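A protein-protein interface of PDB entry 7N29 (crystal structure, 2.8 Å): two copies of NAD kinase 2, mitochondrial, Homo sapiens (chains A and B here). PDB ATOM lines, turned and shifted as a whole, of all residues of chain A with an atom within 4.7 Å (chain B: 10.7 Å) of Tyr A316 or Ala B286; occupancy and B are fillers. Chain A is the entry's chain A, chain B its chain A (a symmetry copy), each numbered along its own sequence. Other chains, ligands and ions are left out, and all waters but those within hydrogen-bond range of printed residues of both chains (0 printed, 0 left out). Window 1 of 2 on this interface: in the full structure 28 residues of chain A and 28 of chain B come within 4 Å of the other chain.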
ATOM      1  N   ASN A 280     -18.752 -17.847   7.549  1.00  0.00           N
ATOM      2  CA  ASN A 280     -18.235 -16.490   7.637  1.00  0.00           C
ATOM      3  C   ASN A 280     -18.122 -15.735   6.316  1.00  0.00           C
ATOM      4  O   ASN A 280     -17.975 -14.514   6.346  1.00  0.00           O
ATOM      5  CB  ASN A 280     -16.859 -16.502   8.308  1.00  0.00           C
ATOM      6  CG  ASN A 280     -16.946 -16.858   9.750  1.00  0.00           C
ATOM      7  OD1 ASN A 280     -17.622 -16.182  10.498  1.00  0.00           O
ATOM      8  ND2 ASN A 280     -16.339 -17.968  10.142  1.00  0.00           N
ATOM      9  N   VAL A 282     -18.836 -13.602   2.963  1.00  0.00           N
ATOM     10  CA  VAL A 282     -19.832 -12.646   2.502  1.00  0.00           C
ATOM     11  C   VAL A 282     -20.026 -12.818   0.998  1.00  0.00           C
ATOM     12  O   VAL A 282     -19.084 -13.095   0.254  1.00  0.00           O
ATOM     13  CB  VAL A 282     -19.439 -11.182   2.810  1.00  0.00           C
ATOM     14  CG1 VAL A 282     -19.506 -10.881   4.296  1.00  0.00           C
ATOM     15  CG2 VAL A 282     -18.048 -10.891   2.258  1.00  0.00           C
ATOM     16  N   VAL A 312     -13.037  -6.839  -3.728  1.00  0.00           N
ATOM     17  CA  VAL A 312     -13.129  -6.644  -2.285  1.00  0.00           C
ATOM     18  C   VAL A 312     -13.741  -7.873  -1.636  1.00  0.00           C
ATOM     19  O   VAL A 312     -13.249  -8.362  -0.611  1.00  0.00           O
ATOM     20  CB  VAL A 312     -13.910  -5.364  -1.946  1.00  0.00           C
ATOM     21  CG1 VAL A 312     -13.081  -4.123  -2.310  1.00  0.00           C
ATOM     22  CG2 VAL A 312     -15.163  -5.319  -2.731  1.00  0.00           C
ATOM     23  N   THR A 313     -14.782  -8.433  -2.258  1.00  0.00           N
ATOM     24  CA  THR A 313     -15.360  -9.664  -1.733  1.00  0.00           C
ATOM     25  C   THR A 313     -14.297 -10.746  -1.603  1.00  0.00           C
ATOM     26  O   THR A 313     -14.097 -11.302  -0.518  1.00  0.00           O
ATOM     27  CB  THR A 313     -16.482 -10.153  -2.648  1.00  0.00           C
ATOM     28  OG1 THR A 313     -17.468  -9.133  -2.792  1.00  0.00           O
ATOM     29  CG2 THR A 313     -17.115 -11.415  -2.080  1.00  0.00           C
ATOM     30  N   ASN A 314     -13.543 -10.991  -2.687  1.00  0.00           N
ATOM     31  CA  ASN A 314     -12.539 -12.050  -2.663  1.00  0.00           C
ATOM     32  C   ASN A 314     -11.445 -11.754  -1.653  1.00  0.00           C
ATOM     33  O   ASN A 314     -11.083 -12.624  -0.859  1.00  0.00           O
ATOM     34  CB  ASN A 314     -11.944 -12.254  -4.054  1.00  0.00           C
ATOM     35  CG  ASN A 314     -12.970 -12.723  -5.056  1.00  0.00           C
ATOM     36  OD1 ASN A 314     -14.054 -13.182  -4.687  1.00  0.00           O
ATOM     37  ND2 ASN A 314     -12.638 -12.621  -6.332  1.00  0.00           N
ATOM     38  N   GLU A 315     -10.970 -10.515  -1.596  1.00  0.00           N
ATOM     39  CA  GLU A 315      -9.971 -10.205  -0.584  1.00  0.00           C
ATOM     40  C   GLU A 315     -10.540 -10.397   0.815  1.00  0.00           C
ATOM     41  O   GLU A 315      -9.863 -10.929   1.700  1.00  0.00           O
ATOM     42  CB  GLU A 315      -9.440  -8.792  -0.766  1.00  0.00           C
ATOM     43  CG  GLU A 315      -8.420  -8.427   0.282  1.00  0.00           C
ATOM     44  CD  GLU A 315      -7.420  -7.394  -0.203  1.00  0.00           C
ATOM     45  OE1 GLU A 315      -7.308  -7.184  -1.439  1.00  0.00           O
ATOM     46  OE2 GLU A 315      -6.732  -6.803   0.659  1.00  0.00           O
ATOM     47  N   TYR A 316     -11.794  -9.999   1.028  1.00  0.00           N
ATOM     48  CA  TYR A 316     -12.409 -10.212   2.331  1.00  0.00           C
ATOM     49  C   TYR A 316     -12.533 -11.699   2.650  1.00  0.00           C
ATOM     50  O   TYR A 316     -12.098 -12.162   3.715  1.00  0.00           O
ATOM     51  CB  TYR A 316     -13.780  -9.546   2.387  1.00  0.00           C
ATOM     52  CG  TYR A 316     -14.444  -9.792   3.715  1.00  0.00           C
ATOM     53  CD1 TYR A 316     -14.216  -8.955   4.773  1.00  0.00           C
ATOM     54  CD2 TYR A 316     -15.261 -10.899   3.926  1.00  0.00           C
ATOM     55  CE1 TYR A 316     -14.792  -9.190   5.987  1.00  0.00           C
ATOM     56  CE2 TYR A 316     -15.831 -11.135   5.140  1.00  0.00           C
ATOM     57  CZ  TYR A 316     -15.591 -10.278   6.168  1.00  0.00           C
ATOM     58  OH  TYR A 316     -16.167 -10.483   7.397  1.00  0.00           O
ATOM     59  N   ASN A 317     -13.135 -12.466   1.738  1.00  0.00           N
ATOM     60  CA  ASN A 317     -13.309 -13.897   1.972  1.00  0.00           C
ATOM     61  C   ASN A 317     -11.974 -14.612   2.148  1.00  0.00           C
ATOM     62  O   ASN A 317     -11.908 -15.626   2.850  1.00  0.00           O
ATOM     63  CB  ASN A 317     -14.090 -14.523   0.817  1.00  0.00           C
ATOM     64  CG  ASN A 317     -15.548 -14.146   0.841  1.00  0.00           C
ATOM     65  OD1 ASN A 317     -16.078 -13.786   1.879  1.00  0.00           O
ATOM     66  ND2 ASN A 317     -16.194 -14.181  -0.315  1.00  0.00           N
ATOM     67  N   GLU A 318     -10.910 -14.115   1.502  1.00  0.00           N
ATOM     68  CA  GLU A 318      -9.581 -14.705   1.674  1.00  0.00           C
ATOM     69  C   GLU A 318      -9.095 -14.598   3.116  1.00  0.00           C
ATOM     70  O   GLU A 318      -8.502 -15.542   3.651  1.00  0.00           O
ATOM     71  CB  GLU A 318      -8.575 -14.023   0.745  1.00  0.00           C
ATOM     72  CG  GLU A 318      -8.460 -14.616  -0.638  1.00  0.00           C
ATOM     73  CD  GLU A 318      -7.761 -15.967  -0.645  1.00  0.00           C
ATOM     74  OE1 GLU A 318      -8.092 -16.790  -1.529  1.00  0.00           O
ATOM     75  OE2 GLU A 318      -6.893 -16.214   0.231  1.00  0.00           O
ATOM     76  N   SER A 319      -9.357 -13.469   3.773  1.00  0.00           N
ATOM     77  CA  SER A 319      -8.894 -13.310   5.145  1.00  0.00           C
ATOM     78  C   SER A 319      -9.515 -14.314   6.107  1.00  0.00           C
ATOM     79  O   SER A 319      -9.038 -14.435   7.240  1.00  0.00           O
ATOM     80  CB  SER A 319      -9.205 -11.900   5.629  1.00  0.00           C
ATOM     81  OG  SER A 319     -10.570 -11.814   6.020  1.00  0.00           O
ATOM     82  N   LEU A 320     -10.579 -15.009   5.696  1.00  0.00           N
ATOM     83  CA  LEU A 320     -11.171 -16.075   6.492  1.00  0.00           C
ATOM     84  C   LEU A 320     -10.370 -17.367   6.447  1.00  0.00           C
ATOM     85  O   LEU A 320     -10.665 -18.268   7.243  1.00  0.00           O
ATOM     86  CB  LEU A 320     -12.601 -16.353   6.028  1.00  0.00           C
ATOM     87  CG  LEU A 320     -13.607 -15.188   6.078  1.00  0.00           C
ATOM     88  CD1 LEU A 320     -14.893 -15.576   5.388  1.00  0.00           C
ATOM     89  CD2 LEU A 320     -13.921 -14.765   7.481  1.00  0.00           C
ATOM     90  N   ARG A 348     -16.020 -13.659  15.933  1.00  0.00           N
ATOM     91  CA  ARG A 348     -15.011 -14.496  15.302  1.00  0.00           C
ATOM     92  C   ARG A 348     -13.625 -13.989  15.676  1.00  0.00           C
ATOM     93  O   ARG A 348     -13.368 -12.787  15.657  1.00  0.00           O
ATOM     94  CB  ARG A 348     -15.209 -14.509  13.787  1.00  0.00           C
ATOM     95  CG  ARG A 348     -14.231 -15.327  13.024  1.00  0.00           C
ATOM     96  CD  ARG A 348     -13.871 -14.577  11.766  1.00  0.00           C
ATOM     97  NE  ARG A 348     -15.072 -14.110  11.084  1.00  0.00           N
ATOM     98  CZ  ARG A 348     -15.100 -13.106  10.213  1.00  0.00           C
ATOM     99  NH1 ARG A 348     -13.984 -12.455   9.912  1.00  0.00           N
ATOM    100  NH2 ARG A 348     -16.250 -12.765   9.640  1.00  0.00           N
ATOM    101  N   ASN B 280     -28.797 -13.329   8.600  1.00  0.00           N
ATOM    102  CA  ASN B 280     -28.405 -12.433   7.523  1.00  0.00           C
ATOM    103  C   ASN B 280     -27.695 -11.152   7.950  1.00  0.00           C
ATOM    104  O   ASN B 280     -27.088 -10.503   7.099  1.00  0.00           O
ATOM    105  CB  ASN B 280     -29.632 -12.054   6.691  1.00  0.00           C
ATOM    106  CG  ASN B 280     -30.156 -13.209   5.912  1.00  0.00           C
ATOM    107  OD1 ASN B 280     -29.435 -13.775   5.116  1.00  0.00           O
ATOM    108  ND2 ASN B 280     -31.380 -13.629   6.192  1.00  0.00           N
ATOM    109  N   ARG B 281     -27.767 -10.741   9.206  1.00  0.00           N
ATOM    110  CA  ARG B 281     -27.131  -9.479   9.564  1.00  0.00           C
ATOM    111  C   ARG B 281     -25.611  -9.547   9.432  1.00  0.00           C
ATOM    112  O   ARG B 281     -25.001 -10.612   9.570  1.00  0.00           O
ATOM    113  CB  ARG B 281     -27.486  -9.079  10.990  1.00  0.00           C
ATOM    114  CG  ARG B 281     -27.033 -10.040  12.048  1.00  0.00           C
ATOM    115  CD  ARG B 281     -27.642  -9.562  13.315  1.00  0.00           C
ATOM    116  NE  ARG B 281     -27.163 -10.246  14.506  1.00  0.00           N
ATOM    117  CZ  ARG B 281     -26.130  -9.812  15.218  1.00  0.00           C
ATOM    118  NH1 ARG B 281     -25.475  -8.718  14.825  1.00  0.00           N
ATOM    119  NH2 ARG B 281     -25.758 -10.466  16.314  1.00  0.00           N
ATOM    120  N   VAL B 282     -25.005  -8.392   9.154  1.00  0.00           N
ATOM    121  CA  VAL B 282     -23.559  -8.232   9.126  1.00  0.00           C
ATOM    122  C   VAL B 282     -23.121  -7.456  10.364  1.00  0.00           C
ATOM    123  O   VAL B 282     -23.807  -6.544  10.829  1.00  0.00           O
ATOM    124  CB  VAL B 282     -23.066  -7.502   7.854  1.00  0.00           C
ATOM    125  CG1 VAL B 282     -23.224  -8.362   6.613  1.00  0.00           C
ATOM    126  CG2 VAL B 282     -23.805  -6.178   7.697  1.00  0.00           C
ATOM    127  N   ALA B 283     -21.931  -7.765  10.855  1.00  0.00           N
ATOM    128  CA  ALA B 283     -21.413  -7.064  12.015  1.00  0.00           C
ATOM    129  C   ALA B 283     -20.724  -5.780  11.588  1.00  0.00           C
ATOM    130  O   ALA B 283     -20.256  -5.653  10.451  1.00  0.00           O
ATOM    131  CB  ALA B 283     -20.437  -7.941  12.793  1.00  0.00           C
ATOM    132  N   THR B 284     -20.694  -4.812  12.512  1.00  0.00           N
ATOM    133  CA  THR B 284     -20.017  -3.548  12.233  1.00  0.00           C
ATOM    134  C   THR B 284     -18.569  -3.781  11.822  1.00  0.00           C
ATOM    135  O   THR B 284     -18.053  -3.075  10.949  1.00  0.00           O
ATOM    136  CB  THR B 284     -20.073  -2.607  13.455  1.00  0.00           C
ATOM    137  OG1 THR B 284     -20.402  -3.339  14.640  1.00  0.00           O
ATOM    138  CG2 THR B 284     -21.117  -1.520  13.263  1.00  0.00           C
ATOM    139  N   GLN B 285     -17.912  -4.789  12.406  1.00  0.00           N
ATOM    140  CA  GLN B 285     -16.534  -5.090  12.033  1.00  0.00           C
ATOM    141  C   GLN B 285     -16.412  -5.576  10.591  1.00  0.00           C
ATOM    142  O   GLN B 285     -15.442  -5.238   9.899  1.00  0.00           O
ATOM    143  CB  GLN B 285     -15.942  -6.116  12.987  1.00  0.00           C
ATOM    144  CG  GLN B 285     -14.472  -6.401  12.723  1.00  0.00           C
ATOM    145  CD  GLN B 285     -13.602  -5.152  12.729  1.00  0.00           C
ATOM    146  OE1 GLN B 285     -13.754  -4.276  13.580  1.00  0.00           O
ATOM    147  NE2 GLN B 285     -12.681  -5.069  11.771  1.00  0.00           N
ATOM    148  N   ALA B 286     -17.357  -6.391  10.121  1.00  0.00           N
ATOM    149  CA  ALA B 286     -17.277  -6.832   8.733  1.00  0.00           C
ATOM    150  C   ALA B 286     -17.450  -5.660   7.787  1.00  0.00           C
ATOM    151  O   ALA B 286     -16.712  -5.526   6.805  1.00  0.00           O
ATOM    152  CB  ALA B 286     -18.313  -7.906   8.439  1.00  0.00           C
ATOM    153  N   VAL B 287     -18.433  -4.810   8.050  1.00  0.00           N
ATOM    154  CA  VAL B 287     -18.588  -3.639   7.207  1.00  0.00           C
ATOM    155  C   VAL B 287     -17.296  -2.833   7.204  1.00  0.00           C
ATOM    156  O   VAL B 287     -16.816  -2.399   6.147  1.00  0.00           O
ATOM    157  CB  VAL B 287     -19.788  -2.804   7.672  1.00  0.00           C
ATOM    158  CG1 VAL B 287     -19.890  -1.573   6.824  1.00  0.00           C
ATOM    159  CG2 VAL B 287     -21.065  -3.641   7.594  1.00  0.00           C
ATOM    160  N   GLU B 288     -16.692  -2.657   8.383  1.00  0.00           N
ATOM    161  CA  GLU B 288     -15.441  -1.914   8.471  1.00  0.00           C
ATOM    162  C   GLU B 288     -14.350  -2.557   7.619  1.00  0.00           C
ATOM    163  O   GLU B 288     -13.597  -1.858   6.930  1.00  0.00           O
ATOM    164  CB  GLU B 288     -15.006  -1.814   9.929  1.00  0.00           C
ATOM    165  CG  GLU B 288     -13.665  -1.142  10.121  1.00  0.00           C
ATOM    166  CD  GLU B 288     -13.449  -0.677  11.549  1.00  0.00           C
ATOM    167  OE1 GLU B 288     -14.337  -0.911  12.402  1.00  0.00           O
ATOM    168  OE2 GLU B 288     -12.372  -0.099  11.821  1.00  0.00           O
ATOM    169  N   ASP B 289     -14.260  -3.892   7.640  1.00  0.00           N
ATOM    170  CA  ASP B 289     -13.265  -4.586   6.825  1.00  0.00           C
ATOM    171  C   ASP B 289     -13.542  -4.375   5.344  1.00  0.00           C
ATOM    172  O   ASP B 289     -12.625  -4.104   4.561  1.00  0.00           O
ATOM    173  CB  ASP B 289     -13.248  -6.086   7.140  1.00  0.00           C
ATOM    174  CG  ASP B 289     -12.714  -6.396   8.531  1.00  0.00           C
ATOM    175  OD1 ASP B 289     -12.250  -5.466   9.219  1.00  0.00           O
ATOM    176  OD2 ASP B 289     -12.744  -7.579   8.932  1.00  0.00           O
ATOM    177  N   VAL B 290     -14.805  -4.522   4.940  1.00  0.00           N
ATOM    178  CA  VAL B 290     -15.164  -4.326   3.540  1.00  0.00           C
ATOM    179  C   VAL B 290     -14.716  -2.950   3.069  1.00  0.00           C
ATOM    180  O   VAL B 290     -14.024  -2.819   2.054  1.00  0.00           O
ATOM    181  CB  VAL B 290     -16.675  -4.528   3.343  1.00  0.00           C
ATOM    182  CG1 VAL B 290     -17.120  -3.877   2.048  1.00  0.00           C
ATOM    183  CG2 VAL B 290     -17.003  -6.005   3.360  1.00  0.00           C
ATOM    184  N   LEU B 291     -15.065  -1.909   3.831  1.00  0.00           N
ATOM    185  CA  LEU B 291     -14.711  -0.539   3.453  1.00  0.00           C
ATOM    186  C   LEU B 291     -13.202  -0.332   3.433  1.00  0.00           C
ATOM    187  O   LEU B 291     -12.661   0.252   2.486  1.00  0.00           O
ATOM    188  CB  LEU B 291     -15.392   0.454   4.399  1.00  0.00           C
ATOM    189  CG  LEU B 291     -16.917   0.379   4.336  1.00  0.00           C
ATOM    190  CD1 LEU B 291     -17.549   1.350   5.293  1.00  0.00           C
ATOM    191  CD2 LEU B 291     -17.351   0.677   2.909  1.00  0.00           C
ATOM    192  N   ASN B 292     -12.502  -0.796   4.474  1.00  0.00           N
ATOM    193  CA  ASN B 292     -11.045  -0.681   4.486  1.00  0.00           C
ATOM    194  C   ASN B 292     -10.448  -1.360   3.260  1.00  0.00           C
ATOM    195  O   ASN B 292      -9.547  -0.815   2.612  1.00  0.00           O
ATOM    196  CB  ASN B 292     -10.471  -1.307   5.756  1.00  0.00           C
ATOM    197  CG  ASN B 292     -10.358  -0.323   6.900  1.00  0.00           C
ATOM    198  OD1 ASN B 292      -9.577   0.628   6.843  1.00  0.00           O
ATOM    199  ND2 ASN B 292     -11.130  -0.560   7.964  1.00  0.00           N
ATOM    200  N   ILE B 293     -10.939  -2.557   2.929  1.00  0.00           N
ATOM    201  CA  ILE B 293     -10.490  -3.226   1.714  1.00  0.00           C
ATOM    202  C   ILE B 293     -10.774  -2.347   0.502  1.00  0.00           C
ATOM    203  O   ILE B 293      -9.900  -2.117  -0.335  1.00  0.00           O
ATOM    204  CB  ILE B 293     -11.143  -4.613   1.589  1.00  0.00           C
ATOM    205  CG1 ILE B 293     -10.595  -5.547   2.665  1.00  0.00           C
ATOM    206  CG2 ILE B 293     -10.865  -5.203   0.243  1.00  0.00           C
ATOM    207  CD1 ILE B 293     -11.426  -6.808   2.863  1.00  0.00           C
ATOM    208  N   ALA B 294     -11.987  -1.805   0.416  1.00  0.00           N
ATOM    209  CA  ALA B 294     -12.320  -0.932  -0.705  1.00  0.00           C
ATOM    210  C   ALA B 294     -11.487   0.348  -0.672  1.00  0.00           C
ATOM    211  O   ALA B 294     -11.047   0.835  -1.723  1.00  0.00           O
ATOM    212  CB  ALA B 294     -13.814  -0.618  -0.701  1.00  0.00           C
ATOM    213  N   LYS B 295     -11.310   0.942   0.516  1.00  0.00           N
ATOM    214  CA  LYS B 295     -10.500   2.156   0.617  1.00  0.00           C
ATOM    215  C   LYS B 295      -9.048   1.868   0.255  1.00  0.00           C
ATOM    216  O   LYS B 295      -8.391   2.679  -0.407  1.00  0.00           O
ATOM    217  CB  LYS B 295     -10.599   2.757   2.022  1.00  0.00           C
ATOM    218  N   ARG B 296      -8.552   0.684   0.638  1.00  0.00           N
ATOM    219  CA  ARG B 296      -7.184   0.263   0.334  1.00  0.00           C
ATOM    220  C   ARG B 296      -7.031  -0.179  -1.114  1.00  0.00           C
ATOM    221  O   ARG B 296      -6.006   0.105  -1.744  1.00  0.00           O
ATOM    222  CB  ARG B 296      -6.788  -0.896   1.244  1.00  0.00           C
ATOM    223  CG  ARG B 296      -5.360  -1.337   1.158  1.00  0.00           C
ATOM    224  CD  ARG B 296      -5.173  -2.620   1.956  1.00  0.00           C
ATOM    225  NE  ARG B 296      -3.788  -3.077   1.902  1.00  0.00           N
ATOM    226  CZ  ARG B 296      -3.312  -4.166   2.501  1.00  0.00           C
ATOM    227  NH1 ARG B 296      -4.100  -4.953   3.228  1.00  0.00           N
ATOM    228  NH2 ARG B 296      -2.032  -4.474   2.348  1.00  0.00           N
ATOM    229  N   GLN B 297      -8.027  -0.889  -1.653  1.00  0.00           N
ATOM    230  CA  GLN B 297      -7.995  -1.284  -3.057  1.00  0.00           C
ATOM    231  C   GLN B 297      -8.405  -0.170  -4.017  1.00  0.00           C
ATOM    232  O   GLN B 297      -8.079  -0.252  -5.206  1.00  0.00           O
ATOM    233  CB  GLN B 297      -8.894  -2.508  -3.298  1.00  0.00           C
ATOM    234  CG  GLN B 297      -8.559  -3.783  -2.503  1.00  0.00           C
ATOM    235  CD  GLN B 297      -7.107  -4.241  -2.643  1.00  0.00           C
ATOM    236  OE1 GLN B 297      -6.295  -4.005  -1.749  1.00  0.00           O
ATOM    237  NE2 GLN B 297      -6.785  -4.928  -3.745  1.00  0.00           N
ATOM    238  N   VAL B 309     -19.292   4.250   9.908  1.00  0.00           N
ATOM    239  CA  VAL B 309     -19.310   2.797   9.747  1.00  0.00           C
ATOM    240  C   VAL B 309     -20.501   2.173  10.465  1.00  0.00           C
ATOM    241  O   VAL B 309     -21.125   1.237   9.959  1.00  0.00           O
ATOM    242  CB  VAL B 309     -17.982   2.178  10.218  1.00  0.00           C
ATOM    243  CG1 VAL B 309     -18.065   0.658  10.220  1.00  0.00           C
ATOM    244  CG2 VAL B 309     -16.863   2.615   9.312  1.00  0.00           C
ATOM    245  N   GLU B 310     -20.826   2.643  11.666  1.00  0.00           N
ATOM    246  CA  GLU B 310     -21.997   2.088  12.328  1.00  0.00           C
ATOM    247  C   GLU B 310     -23.268   2.404  11.562  1.00  0.00           C
ATOM    248  O   GLU B 310     -24.259   1.675  11.692  1.00  0.00           O
ATOM    249  CB  GLU B 310     -22.115   2.586  13.767  1.00  0.00           C
ATOM    250  CG  GLU B 310     -20.989   2.123  14.675  1.00  0.00           C
ATOM    251  CD  GLU B 310     -21.062   2.736  16.061  1.00  0.00           C
ATOM    252  OE1 GLU B 310     -22.187   2.946  16.567  1.00  0.00           O
ATOM    253  OE2 GLU B 310     -19.993   3.008  16.643  1.00  0.00           O
ATOM    254  N   VAL B 312     -23.632   2.609   8.046  1.00  0.00           N
ATOM    255  CA  VAL B 312     -23.823   1.711   6.911  1.00  0.00           C
ATOM    256  C   VAL B 312     -24.260   0.343   7.403  1.00  0.00           C
ATOM    257  O   VAL B 312     -25.194  -0.260   6.857  1.00  0.00           O
ATOM    258  CB  VAL B 312     -22.556   1.635   6.044  1.00  0.00           C
ATOM    259  CG1 VAL B 312     -22.351   2.955   5.283  1.00  0.00           C
ATOM    260  CG2 VAL B 312     -21.373   1.419   6.904  1.00  0.00           C
ATOM    261  N   THR B 313     -23.640  -0.140   8.482  1.00  0.00           N
ATOM    262  CA  THR B 313     -24.071  -1.409   9.056  1.00  0.00           C
ATOM    263  C   THR B 313     -25.557  -1.375   9.385  1.00  0.00           C
ATOM    264  O   THR B 313     -26.325  -2.222   8.916  1.00  0.00           O
ATOM    265  CB  THR B 313     -23.272  -1.717  10.321  1.00  0.00           C
ATOM    266  OG1 THR B 313     -21.878  -1.727  10.021  1.00  0.00           O
ATOM    267  CG2 THR B 313     -23.691  -3.062  10.897  1.00  0.00           C
ATOM    268  N   ASN B 314     -25.993  -0.340  10.122  1.00  0.00           N
ATOM    269  CA  ASN B 314     -27.392  -0.260  10.528  1.00  0.00           C
ATOM    270  C   ASN B 314     -28.311  -0.122   9.328  1.00  0.00           C
ATOM    271  O   ASN B 314     -29.312  -0.834   9.229  1.00  0.00           O
ATOM    272  CB  ASN B 314     -27.602   0.898  11.500  1.00  0.00           C
ATOM    273  CG  ASN B 314     -26.839   0.713  12.790  1.00  0.00           C
ATOM    274  OD1 ASN B 314     -26.387  -0.389  13.106  1.00  0.00           O
ATOM    275  ND2 ASN B 314     -26.698   1.786  13.550  1.00  0.00           N
ATOM    276  N   TYR B 316     -27.702  -1.233   6.364  1.00  0.00           N
ATOM    277  CA  TYR B 316     -27.703  -2.544   5.730  1.00  0.00           C
ATOM    278  C   TYR B 316     -28.578  -3.531   6.498  1.00  0.00           C
ATOM    279  O   TYR B 316     -29.462  -4.181   5.921  1.00  0.00           O
ATOM    280  CB  TYR B 316     -26.279  -3.080   5.618  1.00  0.00           C
ATOM    281  CG  TYR B 316     -26.269  -4.453   5.000  1.00  0.00           C
ATOM    282  CD1 TYR B 316     -26.220  -4.605   3.641  1.00  0.00           C
ATOM    283  CD2 TYR B 316     -26.362  -5.602   5.780  1.00  0.00           C
ATOM    284  CE1 TYR B 316     -26.240  -5.846   3.075  1.00  0.00           C
ATOM    285  CE2 TYR B 316     -26.388  -6.840   5.213  1.00  0.00           C
ATOM    286  CZ  TYR B 316     -26.328  -6.956   3.860  1.00  0.00           C
ATOM    287  OH  TYR B 316     -26.334  -8.193   3.263  1.00  0.00           O
ATOM    288  N   ASN B 317     -28.339  -3.664   7.805  1.00  0.00           N
ATOM    289  CA  ASN B 317     -29.120  -4.598   8.609  1.00  0.00           C
ATOM    290  C   ASN B 317     -30.605  -4.256   8.597  1.00  0.00           C
ATOM    291  O   ASN B 317     -31.443  -5.154   8.734  1.00  0.00           O
ATOM    292  CB  ASN B 317     -28.597  -4.613  10.046  1.00  0.00           C
ATOM    293  CG  ASN B 317     -27.272  -5.318  10.166  1.00  0.00           C
ATOM    294  OD1 ASN B 317     -26.926  -6.135   9.328  1.00  0.00           O
ATOM    295  ND2 ASN B 317     -26.500  -4.970  11.184  1.00  0.00           N
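The guanidinium group of Arg A348 lies within hydrogen-bond range of the side-chain hydroxyl of Tyr A316 (3.2 Å). O of Tyr A316 is in hydrogen-bond range of OG of Ser A319, 2.8 Å away. NE2 of Gln B285 lies within hydrogen-bond range of OD1 of Asp B289 (2.6 Å).
Val A312 touches Ile B293 (CG1 to CG2, 3.5 Å). CA of Ala B294 touches CG1 of Val A312 (3.7 Å). Glu A315 touches Ile B293 (CB to CG2, 3.99 Å). OH of Tyr A316 touches CB of Ala B286, at 3.5 Å. Asp B289 touches Tyr A316. Tyr A316 touches Ile B293 (CA to CD1, 3.6 Å).
OE1 of Glu A315 sits close to NE2 of Gln B297, at 3.3 Å.
Of the 12 printed residues of chain A, 3 touch a printed residue of chain B. Hydrophobic or aromatic side chains of chain B that line the printed part of chain A: Ala B286, Ile B293 and Ala B294.
No residue of chain B comes within 4 Å of Val A282. Printed residues of chain B within 4 Å of Val A312: Ile B293 (3.5 Å) and Ala B294 (3.7 Å). No residue of chain B comes within 4 Å of Thr A313. Printed residues of chain B within 4 Å of Glu A315: Ile B293 (3.99 Å) and Gln B297 (3.2 Å). Asn A317 touches none of the printed residues of chain B. No residue of chain B comes within 4 Å of Ser A319. Glu B288 touches none of the printed residues of chain A. Val B290 touches none of the printed residues of chain A. Of the printed residues of chain A, Ala B294 touches Val A312. The nearest residue of chain B that does not touch Tyr A316 is Val B290 (4.3 Å). The nearest printed residue of chain A that does not touch Ala B286 is Val A282 (5.2 Å).
7 positions are printed for both chains.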
